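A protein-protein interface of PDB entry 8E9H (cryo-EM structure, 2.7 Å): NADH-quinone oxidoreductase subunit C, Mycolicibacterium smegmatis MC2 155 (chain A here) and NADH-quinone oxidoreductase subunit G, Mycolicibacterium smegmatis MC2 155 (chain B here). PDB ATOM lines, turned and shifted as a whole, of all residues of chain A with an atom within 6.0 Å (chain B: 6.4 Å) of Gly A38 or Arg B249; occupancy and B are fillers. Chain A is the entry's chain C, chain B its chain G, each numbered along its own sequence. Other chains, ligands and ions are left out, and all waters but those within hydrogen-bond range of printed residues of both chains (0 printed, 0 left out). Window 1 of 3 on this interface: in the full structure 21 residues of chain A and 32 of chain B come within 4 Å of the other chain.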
ATOM      1  N   ASN A  34      13.813  27.120 -18.429  1.00  0.00           N
ATOM      2  CA  ASN A  34      13.331  26.162 -17.448  1.00  0.00           C
ATOM      3  C   ASN A  34      11.953  25.666 -17.862  1.00  0.00           C
ATOM      4  O   ASN A  34      11.022  26.463 -18.015  1.00  0.00           O
ATOM      5  CB  ASN A  34      13.282  26.802 -16.064  1.00  0.00           C
ATOM      6  CG  ASN A  34      12.846  25.835 -14.998  1.00  0.00           C
ATOM      7  OD1 ASN A  34      12.565  24.670 -15.273  1.00  0.00           O
ATOM      8  ND2 ASN A  34      12.794  26.312 -13.768  1.00  0.00           N
ATOM      9  N   ASP A  36      10.077  23.598 -16.052  1.00  0.00           N
ATOM     10  CA  ASP A  36       9.235  23.504 -14.865  1.00  0.00           C
ATOM     11  C   ASP A  36       8.801  24.885 -14.390  1.00  0.00           C
ATOM     12  O   ASP A  36       8.906  25.865 -15.133  1.00  0.00           O
ATOM     13  CB  ASP A  36       9.979  22.758 -13.756  1.00  0.00           C
ATOM     14  CG  ASP A  36      10.168  21.292 -14.069  1.00  0.00           C
ATOM     15  OD1 ASP A  36       9.313  20.719 -14.774  1.00  0.00           O
ATOM     16  OD2 ASP A  36      11.172  20.712 -13.610  1.00  0.00           O
ATOM     17  N   THR A  37       8.296  24.968 -13.160  1.00  0.00           N
ATOM     18  CA  THR A  37       7.708  26.194 -12.639  1.00  0.00           C
ATOM     19  C   THR A  37       8.726  27.283 -12.327  1.00  0.00           C
ATOM     20  O   THR A  37       8.353  28.460 -12.324  1.00  0.00           O
ATOM     21  CB  THR A  37       6.917  25.888 -11.371  1.00  0.00           C
ATOM     22  OG1 THR A  37       7.820  25.478 -10.339  1.00  0.00           O
ATOM     23  CG2 THR A  37       5.906  24.786 -11.625  1.00  0.00           C
ATOM     24  N   GLY A  38       9.981  26.935 -12.061  1.00  0.00           N
ATOM     25  CA  GLY A  38      10.969  27.943 -11.730  1.00  0.00           C
ATOM     26  C   GLY A  38      11.555  27.788 -10.344  1.00  0.00           C
ATOM     27  O   GLY A  38      10.822  27.688  -9.358  1.00  0.00           O
ATOM     28  N   ASP A  39      12.885  27.773 -10.258  1.00  0.00           N
ATOM     29  CA  ASP A  39      13.546  27.659  -8.965  1.00  0.00           C
ATOM     30  C   ASP A  39      13.477  28.955  -8.175  1.00  0.00           C
ATOM     31  O   ASP A  39      13.535  28.926  -6.943  1.00  0.00           O
ATOM     32  CB  ASP A  39      15.004  27.251  -9.153  1.00  0.00           C
ATOM     33  CG  ASP A  39      15.167  26.130 -10.150  1.00  0.00           C
ATOM     34  OD1 ASP A  39      14.728  25.001  -9.852  1.00  0.00           O
ATOM     35  OD2 ASP A  39      15.736  26.375 -11.233  1.00  0.00           O
ATOM     36  N   THR A  40      13.372  30.089  -8.859  1.00  0.00           N
ATOM     37  CA  THR A  40      13.244  31.388  -8.221  1.00  0.00           C
ATOM     38  C   THR A  40      11.946  32.033  -8.674  1.00  0.00           C
ATOM     39  O   THR A  40      11.625  32.024  -9.865  1.00  0.00           O
ATOM     40  CB  THR A  40      14.429  32.290  -8.561  1.00  0.00           C
ATOM     41  OG1 THR A  40      15.638  31.682  -8.099  1.00  0.00           O
ATOM     42  CG2 THR A  40      14.269  33.642  -7.903  1.00  0.00           C
ATOM     43  N   SER A  41      11.204  32.587  -7.724  1.00  0.00           N
ATOM     44  CA  SER A  41       9.928  33.199  -8.044  1.00  0.00           C
ATOM     45  C   SER A  41      10.125  34.421  -8.929  1.00  0.00           C
ATOM     46  O   SER A  41      11.137  35.119  -8.850  1.00  0.00           O
ATOM     47  CB  SER A  41       9.201  33.596  -6.764  1.00  0.00           C
ATOM     48  OG  SER A  41       8.084  34.412  -7.054  1.00  0.00           O
ATOM     49  N   ARG A 235      16.498  17.028 -13.480  1.00  0.00           N
ATOM     50  CA  ARG A 235      16.247  18.391 -13.913  1.00  0.00           C
ATOM     51  C   ARG A 235      17.111  18.752 -15.114  1.00  0.00           C
ATOM     52  O   ARG A 235      18.194  18.201 -15.319  1.00  0.00           O
ATOM     53  CB  ARG A 235      16.529  19.349 -12.764  1.00  0.00           C
ATOM     54  CG  ARG A 235      15.801  20.649 -12.863  1.00  0.00           C
ATOM     55  CD  ARG A 235      15.615  21.270 -11.501  1.00  0.00           C
ATOM     56  NE  ARG A 235      14.882  22.521 -11.603  1.00  0.00           N
ATOM     57  CZ  ARG A 235      13.632  22.621 -12.027  1.00  0.00           C
ATOM     58  NH1 ARG A 235      12.901  21.550 -12.281  1.00  0.00           N
ATOM     59  NH2 ARG A 235      13.101  23.825 -12.194  1.00  0.00           N
ATOM     60  N   TYR A 237      17.749  22.398 -17.999  1.00  0.00           N
ATOM     61  CA  TYR A 237      17.476  23.798 -18.297  1.00  0.00           C
ATOM     62  C   TYR A 237      17.722  24.092 -19.765  1.00  0.00           C
ATOM     63  O   TYR A 237      18.355  25.088 -20.122  1.00  0.00           O
ATOM     64  CB  TYR A 237      18.322  24.710 -17.416  1.00  0.00           C
ATOM     65  CG  TYR A 237      17.971  24.599 -15.960  1.00  0.00           C
ATOM     66  CD1 TYR A 237      16.987  25.396 -15.402  1.00  0.00           C
ATOM     67  CD2 TYR A 237      18.615  23.686 -15.145  1.00  0.00           C
ATOM     68  CE1 TYR A 237      16.661  25.290 -14.072  1.00  0.00           C
ATOM     69  CE2 TYR A 237      18.296  23.573 -13.816  1.00  0.00           C
ATOM     70  CZ  TYR A 237      17.319  24.377 -13.283  1.00  0.00           C
ATOM     71  OH  TYR A 237      16.997  24.266 -11.954  1.00  0.00           O
ATOM     72  N   GLU B 122      21.079  27.367 -10.422  1.00  0.00           N
ATOM     73  CA  GLU B 122      19.736  27.921 -10.503  1.00  0.00           C
ATOM     74  C   GLU B 122      19.734  29.382 -10.082  1.00  0.00           C
ATOM     75  O   GLU B 122      18.725  29.897  -9.603  1.00  0.00           O
ATOM     76  CB  GLU B 122      18.774  27.113  -9.638  1.00  0.00           C
ATOM     77  CG  GLU B 122      19.199  27.020  -8.187  1.00  0.00           C
ATOM     78  CD  GLU B 122      18.184  26.299  -7.327  1.00  0.00           C
ATOM     79  OE1 GLU B 122      17.650  25.265  -7.774  1.00  0.00           O
ATOM     80  OE2 GLU B 122      17.924  26.762  -6.198  1.00  0.00           O
ATOM     81  N   GLN B 211      12.685  31.345  -1.742  1.00  0.00           N
ATOM     82  CA  GLN B 211      12.415  31.110  -3.153  1.00  0.00           C
ATOM     83  C   GLN B 211      12.385  32.403  -3.952  1.00  0.00           C
ATOM     84  O   GLN B 211      12.478  32.365  -5.182  1.00  0.00           O
ATOM     85  CB  GLN B 211      11.090  30.373  -3.318  1.00  0.00           C
ATOM     86  CG  GLN B 211      10.829  29.901  -4.727  1.00  0.00           C
ATOM     87  CD  GLN B 211       9.568  29.086  -4.836  1.00  0.00           C
ATOM     88  OE1 GLN B 211       9.021  28.634  -3.832  1.00  0.00           O
ATOM     89  NE2 GLN B 211       9.090  28.893  -6.056  1.00  0.00           N
ATOM     90  N   LEU B 232      18.478  16.776  -9.067  1.00  0.00           N
ATOM     91  CA  LEU B 232      17.139  16.738  -8.501  1.00  0.00           C
ATOM     92  C   LEU B 232      16.150  16.165  -9.502  1.00  0.00           C
ATOM     93  O   LEU B 232      16.134  16.560 -10.669  1.00  0.00           O
ATOM     94  CB  LEU B 232      16.689  18.136  -8.094  1.00  0.00           C
ATOM     95  CG  LEU B 232      17.516  18.827  -7.026  1.00  0.00           C
ATOM     96  CD1 LEU B 232      17.113  20.279  -6.927  1.00  0.00           C
ATOM     97  CD2 LEU B 232      17.329  18.129  -5.702  1.00  0.00           C
ATOM     98  N   SER B 234      12.440  16.568 -10.220  1.00  0.00           N
ATOM     99  CA  SER B 234      11.490  17.615  -9.865  1.00  0.00           C
ATOM    100  C   SER B 234      10.157  17.294 -10.515  1.00  0.00           C
ATOM    101  O   SER B 234      10.107  17.025 -11.718  1.00  0.00           O
ATOM    102  CB  SER B 234      11.998  18.980 -10.320  1.00  0.00           C
ATOM    103  OG  SER B 234      11.206  20.021  -9.788  1.00  0.00           O
ATOM    104  N   SER B 235       9.087  17.321  -9.728  1.00  0.00           N
ATOM    105  CA  SER B 235       7.773  16.985 -10.246  1.00  0.00           C
ATOM    106  C   SER B 235       6.737  17.997  -9.779  1.00  0.00           C
ATOM    107  O   SER B 235       6.804  18.470  -8.642  1.00  0.00           O
ATOM    108  CB  SER B 235       7.355  15.583  -9.790  1.00  0.00           C
ATOM    109  OG  SER B 235       8.314  14.617 -10.176  1.00  0.00           O
ATOM    110  N   PRO B 236       5.764  18.341 -10.620  1.00  0.00           N
ATOM    111  CA  PRO B 236       4.632  19.129 -10.130  1.00  0.00           C
ATOM    112  C   PRO B 236       3.888  18.360  -9.050  1.00  0.00           C
ATOM    113  O   PRO B 236       3.842  17.130  -9.058  1.00  0.00           O
ATOM    114  CB  PRO B 236       3.769  19.331 -11.378  1.00  0.00           C
ATOM    115  CG  PRO B 236       4.695  19.150 -12.508  1.00  0.00           C
ATOM    116  CD  PRO B 236       5.676  18.117 -12.070  1.00  0.00           C
ATOM    117  N   SER B 237       3.308  19.098  -8.113  1.00  0.00           N
ATOM    118  CA  SER B 237       2.652  18.477  -6.976  1.00  0.00           C
ATOM    119  C   SER B 237       1.595  19.424  -6.444  1.00  0.00           C
ATOM    120  O   SER B 237       1.523  20.588  -6.837  1.00  0.00           O
ATOM    121  CB  SER B 237       3.654  18.132  -5.874  1.00  0.00           C
ATOM    122  OG  SER B 237       4.649  17.251  -6.354  1.00  0.00           O
ATOM    123  N   ALA B 247      -0.330  24.720  -5.863  1.00  0.00           N
ATOM    124  CA  ALA B 247       0.586  24.071  -6.781  1.00  0.00           C
ATOM    125  C   ALA B 247       1.996  24.177  -6.225  1.00  0.00           C
ATOM    126  O   ALA B 247       2.360  25.178  -5.606  1.00  0.00           O
ATOM    127  CB  ALA B 247       0.506  24.713  -8.161  1.00  0.00           C
ATOM    128  N   GLN B 248       2.790  23.136  -6.435  1.00  0.00           N
ATOM    129  CA  GLN B 248       4.129  23.085  -5.880  1.00  0.00           C
ATOM    130  C   GLN B 248       5.024  22.307  -6.824  1.00  0.00           C
ATOM    131  O   GLN B 248       4.564  21.661  -7.765  1.00  0.00           O
ATOM    132  CB  GLN B 248       4.138  22.436  -4.498  1.00  0.00           C
ATOM    133  CG  GLN B 248       3.698  23.344  -3.386  1.00  0.00           C
ATOM    134  CD  GLN B 248       4.005  22.757  -2.037  1.00  0.00           C
ATOM    135  OE1 GLN B 248       3.835  21.562  -1.819  1.00  0.00           O
ATOM    136  NE2 GLN B 248       4.477  23.587  -1.124  1.00  0.00           N
ATOM    137  N   ARG B 249       6.316  22.371  -6.548  1.00  0.00           N
ATOM    138  CA  ARG B 249       7.320  21.607  -7.270  1.00  0.00           C
ATOM    139  C   ARG B 249       8.133  20.834  -6.248  1.00  0.00           C
ATOM    140  O   ARG B 249       8.906  21.429  -5.494  1.00  0.00           O
ATOM    141  CB  ARG B 249       8.216  22.521  -8.098  1.00  0.00           C
ATOM    142  CG  ARG B 249       8.889  21.834  -9.255  1.00  0.00           C
ATOM    143  CD  ARG B 249       9.982  22.703  -9.821  1.00  0.00           C
ATOM    144  NE  ARG B 249      11.211  22.609  -9.048  1.00  0.00           N
ATOM    145  CZ  ARG B 249      12.185  23.508  -9.083  1.00  0.00           C
ATOM    146  NH1 ARG B 249      12.078  24.615  -9.795  1.00  0.00           N
ATOM    147  NH2 ARG B 249      13.290  23.293  -8.380  1.00  0.00           N
ATOM    148  N   THR B 250       7.934  19.524  -6.204  1.00  0.00           N
ATOM    149  CA  THR B 250       8.645  18.672  -5.266  1.00  0.00           C
ATOM    150  C   THR B 250       9.966  18.246  -5.884  1.00  0.00           C
ATOM    151  O   THR B 250       9.980  17.645  -6.963  1.00  0.00           O
ATOM    152  CB  THR B 250       7.799  17.451  -4.920  1.00  0.00           C
ATOM    153  OG1 THR B 250       6.572  17.871  -4.314  1.00  0.00           O
ATOM    154  CG2 THR B 250       8.541  16.540  -3.971  1.00  0.00           C
ATOM    155  N   ASP B 251      11.070  18.556  -5.213  1.00  0.00           N
ATOM    156  CA  ASP B 251      12.401  18.180  -5.660  1.00  0.00           C
ATOM    157  C   ASP B 251      12.949  17.121  -4.719  1.00  0.00           C
ATOM    158  O   ASP B 251      13.061  17.363  -3.514  1.00  0.00           O
ATOM    159  CB  ASP B 251      13.335  19.389  -5.676  1.00  0.00           C
ATOM    160  CG  ASP B 251      12.885  20.457  -6.640  1.00  0.00           C
ATOM    161  OD1 ASP B 251      12.010  20.172  -7.478  1.00  0.00           O
ATOM    162  OD2 ASP B 251      13.407  21.587  -6.557  1.00  0.00           O
ATOM    163  N   ARG B 259      13.065  19.469  -1.012  1.00  0.00           N
ATOM    164  CA  ARG B 259      12.374  20.740  -0.880  1.00  0.00           C
ATOM    165  C   ARG B 259      11.117  20.708  -1.732  1.00  0.00           C
ATOM    166  O   ARG B 259      10.941  19.836  -2.587  1.00  0.00           O
ATOM    167  CB  ARG B 259      13.269  21.909  -1.292  1.00  0.00           C
ATOM    168  CG  ARG B 259      13.727  21.841  -2.728  1.00  0.00           C
ATOM    169  CD  ARG B 259      14.470  23.089  -3.129  1.00  0.00           C
ATOM    170  NE  ARG B 259      14.853  23.052  -4.533  1.00  0.00           N
ATOM    171  CZ  ARG B 259      15.674  23.919  -5.106  1.00  0.00           C
ATOM    172  NH1 ARG B 259      16.206  24.920  -4.425  1.00  0.00           N
ATOM    173  NH2 ARG B 259      15.964  23.782  -6.396  1.00  0.00           N
ATOM    174  N   ARG B 260      10.242  21.675  -1.482  1.00  0.00           N
ATOM    175  CA  ARG B 260       9.002  21.824  -2.230  1.00  0.00           C
ATOM    176  C   ARG B 260       8.800  23.304  -2.511  1.00  0.00           C
ATOM    177  O   ARG B 260       8.371  24.054  -1.631  1.00  0.00           O
ATOM    178  CB  ARG B 260       7.821  21.236  -1.464  1.00  0.00           C
ATOM    179  CG  ARG B 260       8.013  19.781  -1.108  1.00  0.00           C
ATOM    180  CD  ARG B 260       6.692  19.073  -0.933  1.00  0.00           C
ATOM    181  NE  ARG B 260       5.952  19.584   0.213  1.00  0.00           N
ATOM    182  CZ  ARG B 260       4.949  18.949   0.799  1.00  0.00           C
ATOM    183  NH1 ARG B 260       4.542  17.764   0.379  1.00  0.00           N
ATOM    184  NH2 ARG B 260       4.338  19.515   1.833  1.00  0.00           N
ATOM    185  N   LEU B 261       9.117  23.717  -3.728  1.00  0.00           N
ATOM    186  CA  LEU B 261       8.974  25.106  -4.118  1.00  0.00           C
ATOM    187  C   LEU B 261       7.522  25.419  -4.454  1.00  0.00           C
ATOM    188  O   LEU B 261       6.704  24.527  -4.674  1.00  0.00           O
ATOM    189  CB  LEU B 261       9.872  25.411  -5.311  1.00  0.00           C
ATOM    190  CG  LEU B 261      11.357  25.146  -5.075  1.00  0.00           C
ATOM    191  CD1 LEU B 261      12.163  25.641  -6.248  1.00  0.00           C
ATOM    192  CD2 LEU B 261      11.836  25.796  -3.796  1.00  0.00           C
ATOM    193  N   ALA B 262       7.217  26.711  -4.527  1.00  0.00           N
ATOM    194  CA  ALA B 262       5.846  27.188  -4.639  1.00  0.00           C
ATOM    195  C   ALA B 262       5.192  26.891  -5.977  1.00  0.00           C
ATOM    196  O   ALA B 262       3.969  27.020  -6.081  1.00  0.00           O
ATOM    197  CB  ALA B 262       5.804  28.693  -4.384  1.00  0.00           C
ATOM    198  N   GLY B 263       5.942  26.510  -6.996  1.00  0.00           N
ATOM    199  CA  GLY B 263       5.228  26.317  -8.234  1.00  0.00           C
ATOM    200  C   GLY B 263       4.666  27.639  -8.733  1.00  0.00           C
ATOM    201  O   GLY B 263       5.063  28.723  -8.303  1.00  0.00           O
ATOM    202  N   GLU B 271       2.620  32.313  -6.671  1.00  0.00           N
ATOM    203  CA  GLU B 271       3.948  31.748  -6.475  1.00  0.00           C
ATOM    204  C   GLU B 271       4.339  31.702  -5.005  1.00  0.00           C
ATOM    205  O   GLU B 271       5.506  31.917  -4.674  1.00  0.00           O
ATOM    206  CB  GLU B 271       4.982  32.543  -7.270  1.00  0.00           C
ATOM    207  CG  GLU B 271       4.633  32.686  -8.739  1.00  0.00           C
ATOM    208  CD  GLU B 271       5.819  33.086  -9.591  1.00  0.00           C
ATOM    209  OE1 GLU B 271       6.913  32.520  -9.393  1.00  0.00           O
ATOM    210  OE2 GLU B 271       5.659  33.970 -10.458  1.00  0.00           O
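Hydrophobic or aromatic side chains of chain B within 4 Å of the printed part of chain A: Leu B261.
Among the printed residues, Asp or Glu carboxylates within 4 Å of a Lys or Arg side-chain nitrogen of the other chain: Asp A39 with Arg B249 (2.7 Å) and Asp A39 with Arg B259 (3.9 Å).
The guanidinium group of Arg B249 lies close to the backbone carbonyl oxygen of Gly A38.
The guanidinium group (NH1) of Arg A235 sits close to the side-chain hydroxyl (OG) of Ser B234 (3.4 Å).
NH2 of Arg A235 lies close to NH1 of Arg B249.
The side-chain hydroxyl (OG) of Ser A41 sits at hydrogen-bond distance from the side-chain carboxylate (OE1) of Glu B271 (3.2 Å).
The side-chain carboxylate (OD1) of Asp A39 is in salt-bridge range of the guanidinium group (NH2) of Arg B249 (2.7 Å).
OD1 of Asp A39 lies within salt-bridge range of NH2 of Arg B259.
N of Arg A235 is in hydrogen-bond range of O of Leu B232 (2.9 Å).
O of Gln B211 lies within hydrogen-bond range of N of Ser A41, 2.9 Å away.
Among the printed residues, merely in contact across the chains: Thr A40 with Gln B211, Thr A37 with Gly B263, Asp A39 with Glu B122, Thr A37 with Arg B249, Asp A39 with Leu B261, Asp A39 with Gln B211, Asp A36 with Ser B234, Thr A40 with Glu B122, Gly A38 with Gln B211, Asp A36 with Arg B249 and Gly A38 with Leu B261.
Gly A38 touches just these residues of chain B: Gln B211, Arg B249 and Leu B261.
Of chain A, only Asp A36, Thr A37, Gly A38, Asp A39 and Arg A235 come within 4 Å of Arg B249.
Of the printed residues of chain B, Asp A39 touches Glu B122, Gln B211, Arg B249, Arg B259 and Leu B261.
Of the printed residues of chain A, Ser B234 touches Asp A36 and Arg A235.
Printed residues of chain A within 4 Å of Gly B263: Thr A37.
Printed residues of chain A within 4 Å of Leu B232: Arg A235.
Of the printed residues of chain B, Asp A36 touches Ser B234 and Arg B249.
Asp B251 touches none of the printed residues of chain A.
The nearest residue of chain B that does not touch Gly A38 is Gly B263 (5.5 Å).
The nearest printed residue of chain A that does not touch Ser B234 is Asp A39 (6.1 Å).
The side-chain hydroxyl of Ser B234 sits at hydrogen-bond distance from the guanidinium group of Arg B249, at 2.7 Å.
The side-chain carboxylate (OD2) of Asp B251 is in salt-bridge range of the guanidinium group (NH2) of Arg B249.
The backbone carbonyl oxygen (O) of Leu B261 sits at hydrogen-bond distance from the backbone NH (N) of Arg B249 (2.9 Å).
OE1 of Glu B122 lies within salt-bridge range of NH2 of Arg B259, at 2.6 Å.
The backbone NH of Gly A38 sits close to the side-chain amide nitrogen of Asn A34.
The side-chain amide oxygen (OE1) of Gln B211 is in hydrogen-bond range of the backbone NH (N) of Ala B262.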
